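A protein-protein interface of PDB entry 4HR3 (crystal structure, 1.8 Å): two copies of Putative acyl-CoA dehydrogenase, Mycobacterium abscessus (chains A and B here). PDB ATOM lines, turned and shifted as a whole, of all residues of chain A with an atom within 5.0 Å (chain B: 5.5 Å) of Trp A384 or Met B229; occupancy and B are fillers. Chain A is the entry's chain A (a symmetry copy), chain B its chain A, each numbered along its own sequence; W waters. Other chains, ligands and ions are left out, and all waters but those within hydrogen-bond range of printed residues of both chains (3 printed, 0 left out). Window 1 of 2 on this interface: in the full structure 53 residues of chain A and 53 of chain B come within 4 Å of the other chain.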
ATOM      1  N   MET A 229     -24.319   7.200  20.556  1.00  0.00           N
ATOM      2  CA  MET A 229     -24.648   7.376  19.130  1.00  0.00           C
ATOM      3  C   MET A 229     -26.147   7.452  18.879  1.00  0.00           C
ATOM      4  O   MET A 229     -26.673   6.746  17.998  1.00  0.00           O
ATOM      5  CB  MET A 229     -24.109   6.222  18.281  1.00  0.00           C
ATOM      6  CG  MET A 229     -22.759   6.507  17.684  1.00  0.00           C
ATOM      7  SD  MET A 229     -21.473   6.352  18.928  1.00  0.00           S
ATOM      8  CE  MET A 229     -20.056   6.637  17.899  1.00  0.00           C
ATOM      9  N   GLY A 230     -26.869   8.261  19.618  1.00  0.00           N
ATOM     10  CA  GLY A 230     -28.329   8.317  19.286  1.00  0.00           C
ATOM     11  C   GLY A 230     -29.218   7.201  19.838  1.00  0.00           C
ATOM     12  O   GLY A 230     -30.455   7.316  19.761  1.00  0.00           O
ATOM     13  N   PHE A 231     -28.626   6.132  20.381  1.00  0.00           N
ATOM     14  CA  PHE A 231     -29.389   5.064  21.046  1.00  0.00           C
ATOM     15  C   PHE A 231     -29.553   5.386  22.529  1.00  0.00           C
ATOM     16  O   PHE A 231     -28.578   5.732  23.194  1.00  0.00           O
ATOM     17  CB  PHE A 231     -28.691   3.711  20.933  1.00  0.00           C
ATOM     18  CG  PHE A 231     -28.667   3.142  19.533  1.00  0.00           C
ATOM     19  CD1 PHE A 231     -29.804   2.550  18.990  1.00  0.00           C
ATOM     20  CD2 PHE A 231     -27.524   3.186  18.772  1.00  0.00           C
ATOM     21  CE1 PHE A 231     -29.782   2.011  17.712  1.00  0.00           C
ATOM     22  CE2 PHE A 231     -27.498   2.644  17.490  1.00  0.00           C
ATOM     23  CZ  PHE A 231     -28.625   2.057  16.958  1.00  0.00           C
ATOM     24  N   GLN A 359     -16.230  -5.172  17.653  1.00  0.00           N
ATOM     25  CA  GLN A 359     -16.392  -3.956  16.876  1.00  0.00           C
ATOM     26  C   GLN A 359     -16.009  -4.180  15.415  1.00  0.00           C
ATOM     27  O   GLN A 359     -16.725  -3.750  14.495  1.00  0.00           O
ATOM     28  CB  GLN A 359     -15.546  -2.823  17.464  1.00  0.00           C
ATOM     29  CG  GLN A 359     -15.733  -1.498  16.736  1.00  0.00           C
ATOM     30  CD  GLN A 359     -14.910  -0.363  17.310  1.00  0.00           C
ATOM     31  OE1 GLN A 359     -14.696  -0.275  18.517  1.00  0.00           O
ATOM     32  NE2 GLN A 359     -14.503   0.562  16.443  1.00  0.00           N
ATOM     33  N   ILE A 362     -18.475  -6.594  13.546  1.00  0.00           N
ATOM     34  CA  ILE A 362     -19.741  -5.924  13.314  1.00  0.00           C
ATOM     35  C   ILE A 362     -19.574  -4.881  12.196  1.00  0.00           C
ATOM     36  O   ILE A 362     -20.420  -4.790  11.329  1.00  0.00           O
ATOM     37  CB  ILE A 362     -20.307  -5.298  14.599  1.00  0.00           C
ATOM     38  CG1 ILE A 362     -20.575  -6.383  15.657  1.00  0.00           C
ATOM     39  CG2 ILE A 362     -21.576  -4.516  14.265  1.00  0.00           C
ATOM     40  CD1 ILE A 362     -20.611  -5.875  17.096  1.00  0.00           C
ATOM     41  N   ASP A 363     -18.479  -4.125  12.195  1.00  0.00           N
ATOM     42  CA  ASP A 363     -18.289  -3.141  11.145  1.00  0.00           C
ATOM     43  C   ASP A 363     -18.215  -3.799   9.770  1.00  0.00           C
ATOM     44  O   ASP A 363     -18.749  -3.263   8.792  1.00  0.00           O
ATOM     45  CB  ASP A 363     -17.057  -2.275  11.388  1.00  0.00           C
ATOM     46  CG  ASP A 363     -17.109  -1.019  10.593  1.00  0.00           C
ATOM     47  OD1 ASP A 363     -18.219  -0.454  10.517  1.00  0.00           O
ATOM     48  OD2 ASP A 363     -16.067  -0.623  10.025  1.00  0.00           O
ATOM     49  N   ILE A 366     -21.937  -4.772   8.885  1.00  0.00           N
ATOM     50  CA  ILE A 366     -22.635  -3.587   8.442  1.00  0.00           C
ATOM     51  C   ILE A 366     -22.304  -3.289   6.978  1.00  0.00           C
ATOM     52  O   ILE A 366     -23.208  -3.049   6.179  1.00  0.00           O
ATOM     53  CB  ILE A 366     -22.264  -2.380   9.325  1.00  0.00           C
ATOM     54  CG1 ILE A 366     -22.877  -2.566  10.714  1.00  0.00           C
ATOM     55  CG2 ILE A 366     -22.675  -1.058   8.697  1.00  0.00           C
ATOM     56  CD1 ILE A 366     -22.465  -1.528  11.725  1.00  0.00           C
ATOM     57  N   LEU A 374     -26.722   0.289   8.503  1.00  0.00           N
ATOM     58  CA  LEU A 374     -26.692   1.378   9.470  1.00  0.00           C
ATOM     59  C   LEU A 374     -28.066   1.613  10.112  1.00  0.00           C
ATOM     60  O   LEU A 374     -28.174   2.386  11.074  1.00  0.00           O
ATOM     61  CB  LEU A 374     -26.223   2.672   8.817  1.00  0.00           C
ATOM     62  CG  LEU A 374     -24.814   2.608   8.227  1.00  0.00           C
ATOM     63  CD1 LEU A 374     -24.554   3.853   7.393  1.00  0.00           C
ATOM     64  CD2 LEU A 374     -23.816   2.486   9.335  1.00  0.00           C
ATOM     65  N   LEU A 380     -27.475  -4.861  13.712  1.00  0.00           N
ATOM     66  CA  LEU A 380     -26.027  -4.622  13.583  1.00  0.00           C
ATOM     67  C   LEU A 380     -25.582  -3.237  14.056  1.00  0.00           C
ATOM     68  O   LEU A 380     -24.528  -3.097  14.694  1.00  0.00           O
ATOM     69  CB  LEU A 380     -25.600  -4.835  12.131  1.00  0.00           C
ATOM     70  CG  LEU A 380     -25.937  -6.202  11.531  1.00  0.00           C
ATOM     71  CD1 LEU A 380     -25.550  -6.230  10.067  1.00  0.00           C
ATOM     72  CD2 LEU A 380     -25.234  -7.315  12.297  1.00  0.00           C
ATOM     73  N   ALA A 381     -26.359  -2.218  13.730  1.00  0.00           N
ATOM     74  CA  ALA A 381     -26.008  -0.848  14.104  1.00  0.00           C
ATOM     75  C   ALA A 381     -25.958  -0.719  15.635  1.00  0.00           C
ATOM     76  O   ALA A 381     -24.995  -0.193  16.189  1.00  0.00           O
ATOM     77  CB  ALA A 381     -26.977   0.152  13.481  1.00  0.00           C
ATOM     78  N   ALA A 382     -26.980  -1.246  16.310  1.00  0.00           N
ATOM     79  CA  ALA A 382     -27.027  -1.231  17.757  1.00  0.00           C
ATOM     80  C   ALA A 382     -25.883  -2.068  18.326  1.00  0.00           C
ATOM     81  O   ALA A 382     -25.242  -1.681  19.324  1.00  0.00           O
ATOM     82  CB  ALA A 382     -28.378  -1.746  18.250  1.00  0.00           C
ATOM     83  N   ALA A 383     -25.608  -3.200  17.682  1.00  0.00           N
ATOM     84  CA  ALA A 383     -24.505  -4.062  18.112  1.00  0.00           C
ATOM     85  C   ALA A 383     -23.175  -3.332  18.067  1.00  0.00           C
ATOM     86  O   ALA A 383     -22.368  -3.418  19.012  1.00  0.00           O
ATOM     87  CB  ALA A 383     -24.437  -5.321  17.262  1.00  0.00           C
ATOM     88  N   TRP A 384     -22.933  -2.615  16.973  1.00  0.00           N
ATOM     89  CA  TRP A 384     -21.669  -1.879  16.859  1.00  0.00           C
ATOM     90  C   TRP A 384     -21.487  -0.945  18.063  1.00  0.00           C
ATOM     91  O   TRP A 384     -20.405  -0.886  18.681  1.00  0.00           O
ATOM     92  CB  TRP A 384     -21.580  -1.087  15.541  1.00  0.00           C
ATOM     93  CG  TRP A 384     -20.241  -0.430  15.403  1.00  0.00           C
ATOM     94  CD1 TRP A 384     -19.155  -0.929  14.769  1.00  0.00           C
ATOM     95  CD2 TRP A 384     -19.849   0.819  15.956  1.00  0.00           C
ATOM     96  NE1 TRP A 384     -18.092  -0.062  14.880  1.00  0.00           N
ATOM     97  CE2 TRP A 384     -18.495   1.019  15.618  1.00  0.00           C
ATOM     98  CE3 TRP A 384     -20.515   1.806  16.702  1.00  0.00           C
ATOM     99  CZ2 TRP A 384     -17.798   2.168  15.984  1.00  0.00           C
ATOM    100  CZ3 TRP A 384     -19.821   2.950  17.057  1.00  0.00           C
ATOM    101  CH2 TRP A 384     -18.480   3.117  16.711  1.00  0.00           C
ATOM    102  N   VAL A 385     -22.537  -0.209  18.390  1.00  0.00           N
ATOM    103  CA  VAL A 385     -22.482   0.760  19.470  1.00  0.00           C
ATOM    104  C   VAL A 385     -22.259   0.051  20.788  1.00  0.00           C
ATOM    105  O   VAL A 385     -21.498   0.527  21.644  1.00  0.00           O
ATOM    106  CB  VAL A 385     -23.762   1.606  19.519  1.00  0.00           C
ATOM    107  CG1 VAL A 385     -23.753   2.519  20.732  1.00  0.00           C
ATOM    108  CG2 VAL A 385     -23.895   2.422  18.250  1.00  0.00           C
ATOM    109  N   ASN A 386     -22.886  -1.106  20.949  1.00  0.00           N
ATOM    110  CA  ASN A 386     -22.663  -1.888  22.150  1.00  0.00           C
ATOM    111  C   ASN A 386     -21.196  -2.286  22.329  1.00  0.00           C
ATOM    112  O   ASN A 386     -20.630  -2.102  23.400  1.00  0.00           O
ATOM    113  CB  ASN A 386     -23.533  -3.115  22.185  1.00  0.00           C
ATOM    114  CG  ASN A 386     -23.399  -3.838  23.498  1.00  0.00           C
ATOM    115  OD1 ASN A 386     -23.919  -3.371  24.523  1.00  0.00           O
ATOM    116  ND2 ASN A 386     -22.610  -4.871  23.527  1.00  0.00           N
ATOM    117  N   ALA A 387     -20.579  -2.822  21.268  1.00  0.00           N
ATOM    118  CA  ALA A 387     -19.189  -3.227  21.349  1.00  0.00           C
ATOM    119  C   ALA A 387     -18.307  -2.003  21.560  1.00  0.00           C
ATOM    120  O   ALA A 387     -17.381  -2.035  22.373  1.00  0.00           O
ATOM    121  CB  ALA A 387     -18.770  -3.982  20.099  1.00  0.00           C
ATOM    122  N   ARG A 388     -18.597  -0.921  20.833  1.00  0.00           N
ATOM    123  CA  ARG A 388     -17.798   0.310  20.965  1.00  0.00           C
ATOM    124  C   ARG A 388     -17.811   0.838  22.404  1.00  0.00           C
ATOM    125  O   ARG A 388     -16.772   1.238  22.963  1.00  0.00           O
ATOM    126  CB  ARG A 388     -18.357   1.416  20.046  1.00  0.00           C
ATOM    127  CG  ARG A 388     -17.624   2.754  20.158  1.00  0.00           C
ATOM    128  CD  ARG A 388     -16.238   2.586  19.638  1.00  0.00           C
ATOM    129  NE  ARG A 388     -15.342   3.725  19.779  1.00  0.00           N
ATOM    130  CZ  ARG A 388     -14.630   4.005  20.871  1.00  0.00           C
ATOM    131  NH1 ARG A 388     -14.769   3.285  21.979  1.00  0.00           N
ATOM    132  NH2 ARG A 388     -13.757   5.004  20.841  1.00  0.00           N
ATOM    133  N   ALA A 389     -18.991   0.829  23.002  1.00  0.00           N
ATOM    134  CA  ALA A 389     -19.166   1.327  24.354  1.00  0.00           C
ATOM    135  C   ALA A 389     -18.420   0.480  25.366  1.00  0.00           C
ATOM    136  O   ALA A 389     -17.955   0.984  26.383  1.00  0.00           O
ATOM    137  CB  ALA A 389     -20.653   1.367  24.695  1.00  0.00           C
ATOM    138  N   PRO B 227     -33.023   5.621  10.328  1.00  0.00           N
ATOM    139  CA  PRO B 227     -31.925   5.982  11.232  1.00  0.00           C
ATOM    140  C   PRO B 227     -30.588   5.525  10.699  1.00  0.00           C
ATOM    141  O   PRO B 227     -30.535   4.540   9.956  1.00  0.00           O
ATOM    142  CB  PRO B 227     -32.238   5.178  12.499  1.00  0.00           C
ATOM    143  CG  PRO B 227     -32.875   3.945  11.964  1.00  0.00           C
ATOM    144  CD  PRO B 227     -33.659   4.359  10.738  1.00  0.00           C
ATOM    145  N   THR B 228     -29.512   6.211  11.102  1.00  0.00           N
ATOM    146  CA  THR B 228     -28.134   5.744  10.925  1.00  0.00           C
ATOM    147  C   THR B 228     -27.601   5.694  12.347  1.00  0.00           C
ATOM    148  O   THR B 228     -27.455   6.732  12.967  1.00  0.00           O
ATOM    149  CB  THR B 228     -27.292   6.745  10.105  1.00  0.00           C
ATOM    150  OG1 THR B 228     -27.322   8.019  10.757  1.00  0.00           O
ATOM    151  CG2 THR B 228     -27.850   6.919   8.759  1.00  0.00           C
ATOM    152  N   MET B 229     -27.385   4.491  12.887  1.00  0.00           N
ATOM    153  CA  MET B 229     -27.085   4.327  14.321  1.00  0.00           C
ATOM    154  C   MET B 229     -27.990   5.164  15.211  1.00  0.00           C
ATOM    155  O   MET B 229     -27.504   5.884  16.102  1.00  0.00           O
ATOM    156  CB  MET B 229     -25.643   4.728  14.644  1.00  0.00           C
ATOM    157  CG  MET B 229     -24.688   3.567  14.629  1.00  0.00           C
ATOM    158  SD  MET B 229     -24.304   3.088  12.941  1.00  0.00           S
ATOM    159  CE  MET B 229     -23.116   1.814  13.278  1.00  0.00           C
ATOM    160  N   GLY B 230     -29.286   5.121  15.008  1.00  0.00           N
ATOM    161  CA  GLY B 230     -30.120   5.936  15.950  1.00  0.00           C
ATOM    162  C   GLY B 230     -30.238   7.435  15.666  1.00  0.00           C
ATOM    163  O   GLY B 230     -31.076   8.108  16.294  1.00  0.00           O
ATOM    164  N   PHE B 231     -29.424   7.970  14.749  1.00  0.00           N
ATOM    165  CA  PHE B 231     -29.540   9.372  14.318  1.00  0.00           C
ATOM    166  C   PHE B 231     -30.496   9.475  13.132  1.00  0.00           C
ATOM    167  O   PHE B 231     -30.374   8.712  12.175  1.00  0.00           O
ATOM    168  CB  PHE B 231     -28.194   9.948  13.887  1.00  0.00           C
ATOM    169  CG  PHE B 231     -27.210  10.134  15.019  1.00  0.00           C
ATOM    170  CD1 PHE B 231     -27.338  11.206  15.899  1.00  0.00           C
ATOM    171  CD2 PHE B 231     -26.166   9.260  15.200  1.00  0.00           C
ATOM    172  CE1 PHE B 231     -26.427  11.392  16.929  1.00  0.00           C
ATOM    173  CE2 PHE B 231     -25.249   9.443  16.231  1.00  0.00           C
ATOM    174  CZ  PHE B 231     -25.378  10.508  17.097  1.00  0.00           C
ATOM    175  N   ASP B 363     -12.872   8.085  15.841  1.00  0.00           N
ATOM    176  CA  ASP B 363     -12.905   7.042  16.849  1.00  0.00           C
ATOM    177  C   ASP B 363     -11.845   7.269  17.922  1.00  0.00           C
ATOM    178  O   ASP B 363     -12.097   7.031  19.109  1.00  0.00           O
ATOM    179  CB  ASP B 363     -12.757   5.651  16.239  1.00  0.00           C
ATOM    180  CG  ASP B 363     -13.229   4.594  17.173  1.00  0.00           C
ATOM    181  OD1 ASP B 363     -14.266   4.844  17.820  1.00  0.00           O
ATOM    182  OD2 ASP B 363     -12.554   3.546  17.286  1.00  0.00           O
ATOM    183  N   TRP B 384     -18.785  10.513  13.818  1.00  0.00           N
ATOM    184  CA  TRP B 384     -18.378   9.143  13.488  1.00  0.00           C
ATOM    185  C   TRP B 384     -19.371   8.517  12.499  1.00  0.00           C
ATOM    186  O   TRP B 384     -18.980   7.897  11.489  1.00  0.00           O
ATOM    187  CB  TRP B 384     -18.240   8.264  14.745  1.00  0.00           C
ATOM    188  CG  TRP B 384     -17.725   6.903  14.390  1.00  0.00           C
ATOM    189  CD1 TRP B 384     -16.434   6.499  14.393  1.00  0.00           C
ATOM    190  CD2 TRP B 384     -18.494   5.797  13.938  1.00  0.00           C
ATOM    191  NE1 TRP B 384     -16.337   5.192  13.974  1.00  0.00           N
ATOM    192  CE2 TRP B 384     -17.597   4.742  13.677  1.00  0.00           C
ATOM    193  CE3 TRP B 384     -19.868   5.585  13.734  1.00  0.00           C
ATOM    194  CZ2 TRP B 384     -18.025   3.491  13.240  1.00  0.00           C
ATOM    195  CZ3 TRP B 384     -20.290   4.337  13.306  1.00  0.00           C
ATOM    196  CH2 TRP B 384     -19.377   3.314  13.054  1.00  0.00           C
ATOM    197  N   VAL B 385     -20.653   8.667  12.792  1.00  0.00           N
ATOM    198  CA  VAL B 385     -21.696   8.072  11.974  1.00  0.00           C
ATOM    199  C   VAL B 385     -21.686   8.693  10.594  1.00  0.00           C
ATOM    200  O   VAL B 385     -21.865   7.996   9.583  1.00  0.00           O
ATOM    201  CB  VAL B 385     -23.073   8.236  12.631  1.00  0.00           C
ATOM    202  CG1 VAL B 385     -24.170   7.736  11.707  1.00  0.00           C
ATOM    203  CG2 VAL B 385     -23.115   7.486  13.946  1.00  0.00           C
ATOM    204  N   ARG B 388     -18.730   7.152   8.790  1.00  0.00           N
ATOM    205  CA  ARG B 388     -19.042   5.735   8.529  1.00  0.00           C
ATOM    206  C   ARG B 388     -20.010   5.580   7.351  1.00  0.00           C
ATOM    207  O   ARG B 388     -19.833   4.718   6.469  1.00  0.00           O
ATOM    208  CB  ARG B 388     -19.693   5.088   9.770  1.00  0.00           C
ATOM    209  CG  ARG B 388     -20.105   3.629   9.572  1.00  0.00           C
ATOM    210  CD  ARG B 388     -18.876   2.803   9.398  1.00  0.00           C
ATOM    211  NE  ARG B 388     -19.071   1.398   9.070  1.00  0.00           N
ATOM    212  CZ  ARG B 388     -19.264   0.921   7.841  1.00  0.00           C
ATOM    213  NH1 ARG B 388     -19.388   1.741   6.802  1.00  0.00           N
ATOM    214  NH2 ARG B 388     -19.312  -0.392   7.651  1.00  0.00           N
HETATM  215  O   HOH W   1     -31.739   9.811  19.148  1.00  0.00           O
HETATM  216  O   HOH W   2     -33.197   6.906  17.812  1.00  0.00           O
HETATM  217  O   HOH W   3     -29.720   2.788  13.320  1.00  0.00           O
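The backbone NH of Met B229 sits at hydrogen-bond distance from the backbone carbonyl oxygen of Leu A374 (2.9 Å). OD1 of Asp B363 lies within salt-bridge range of NE of Arg A388. The side-chain carboxylate (OD1) of Asp A363 lies within salt-bridge range of the guanidinium group (NE) of Arg B388 (2.5 Å). The backbone carbonyl oxygen (O) of Met A229 lies close to the backbone carbonyl oxygen (O) of Met B229. O of Pro B227 sits close to O of Leu A374.
The backbone carbonyl oxygen (O) of Phe B231 is in hydrogen-bond range of the side-chain hydroxyl (OG1) of Thr B228 (3.4 Å).
CG of Met A229 touches CG2 of Val B385, at 3.9 Å. Gly A230 touches Gly B230. N of Gly A230 touches CZ of Phe B231, 3.7 Å away. Phe A231 touches Met B229. Ile A366 touches Met B229 (CD1 to CE, 3.7 Å). Leu A374 touches Thr B228 (O to CA, 3.4 Å). CG of Arg B388 touches CD2 of Leu A374 (3.9 Å). CE of Met B229 touches CB of Trp A384, 3.99 Å away. Trp A384 touches Trp B384. Val A385 touches Met B229.
Printed residues of chain B within 4 Å of Trp A384: Met B229 and Trp B384. Printed residues of chain A within 4 Å of Met B229: Met A229, Phe A231, Ile A366, Leu A374, Trp A384 and Val A385. Printed residues of chain A within 4 Å of Val B385: Met A229 (3.9 Å). Printed residues of chain A within 4 Å of Gly B230: Gly A230 (3.6 Å) and Phe A231 (3.7 Å). The nearest printed residue of chain A that does not touch Met B229 is Ala A381 (4.004 Å). The nearest printed residue of chain B that does not touch Gln A359 is Trp B384 (5.6 Å).
Hydrophobic or aromatic side chains of chain A that line the printed part of chain B: Met A229, Phe A231, Ile A366, Leu A374, Trp A384 and Val A385. Of the 9 printed residues of chain B, 9 touch a printed residue of chain A. Printed residues of chain B that touch a printed residue of chain A: Pro B227, Thr B228, Met B229, Gly B230, Phe B231, Asp B363, Trp B384, Val B385 and Arg B388. Hydrophobic or aromatic side chains of chain B that line the printed part of chain A: Met B229, Phe B231, Trp B384 and Val B385.
Met A229 touches Trp B384, and with the chains exchanged Trp A384 touches Met B229. Met A229 touches Val B385, and with the chains exchanged Val A385 touches Met B229. Gly A230 touches its own counterpart, Gly B230. Asp A363 touches Arg B388, and with the chains exchanged Arg A388 touches Asp B363. 7 positions are printed for both chains. Of the 20 pairs that touch across the chains among the printed residues, 13 have their exchanged pair printed and touching as well.
Water W3 lies within hydrogen-bond range of the backbone carbonyl oxygen of Leu A374 (2.8 Å), the backbone NH of Gly B230 (2.9 Å) and the backbone NH of Met B229 (2.9 Å). Water W2 lies within hydrogen-bond range of the backbone carbonyl oxygen of Gly B230 and the backbone carbonyl oxygen of Gly A230. Water W1 lies within hydrogen-bond range of the backbone carbonyl oxygen (O) of Gly A230 (2.9 Å) and the backbone carbonyl oxygen (O) of Gly B230 (3.4 Å).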
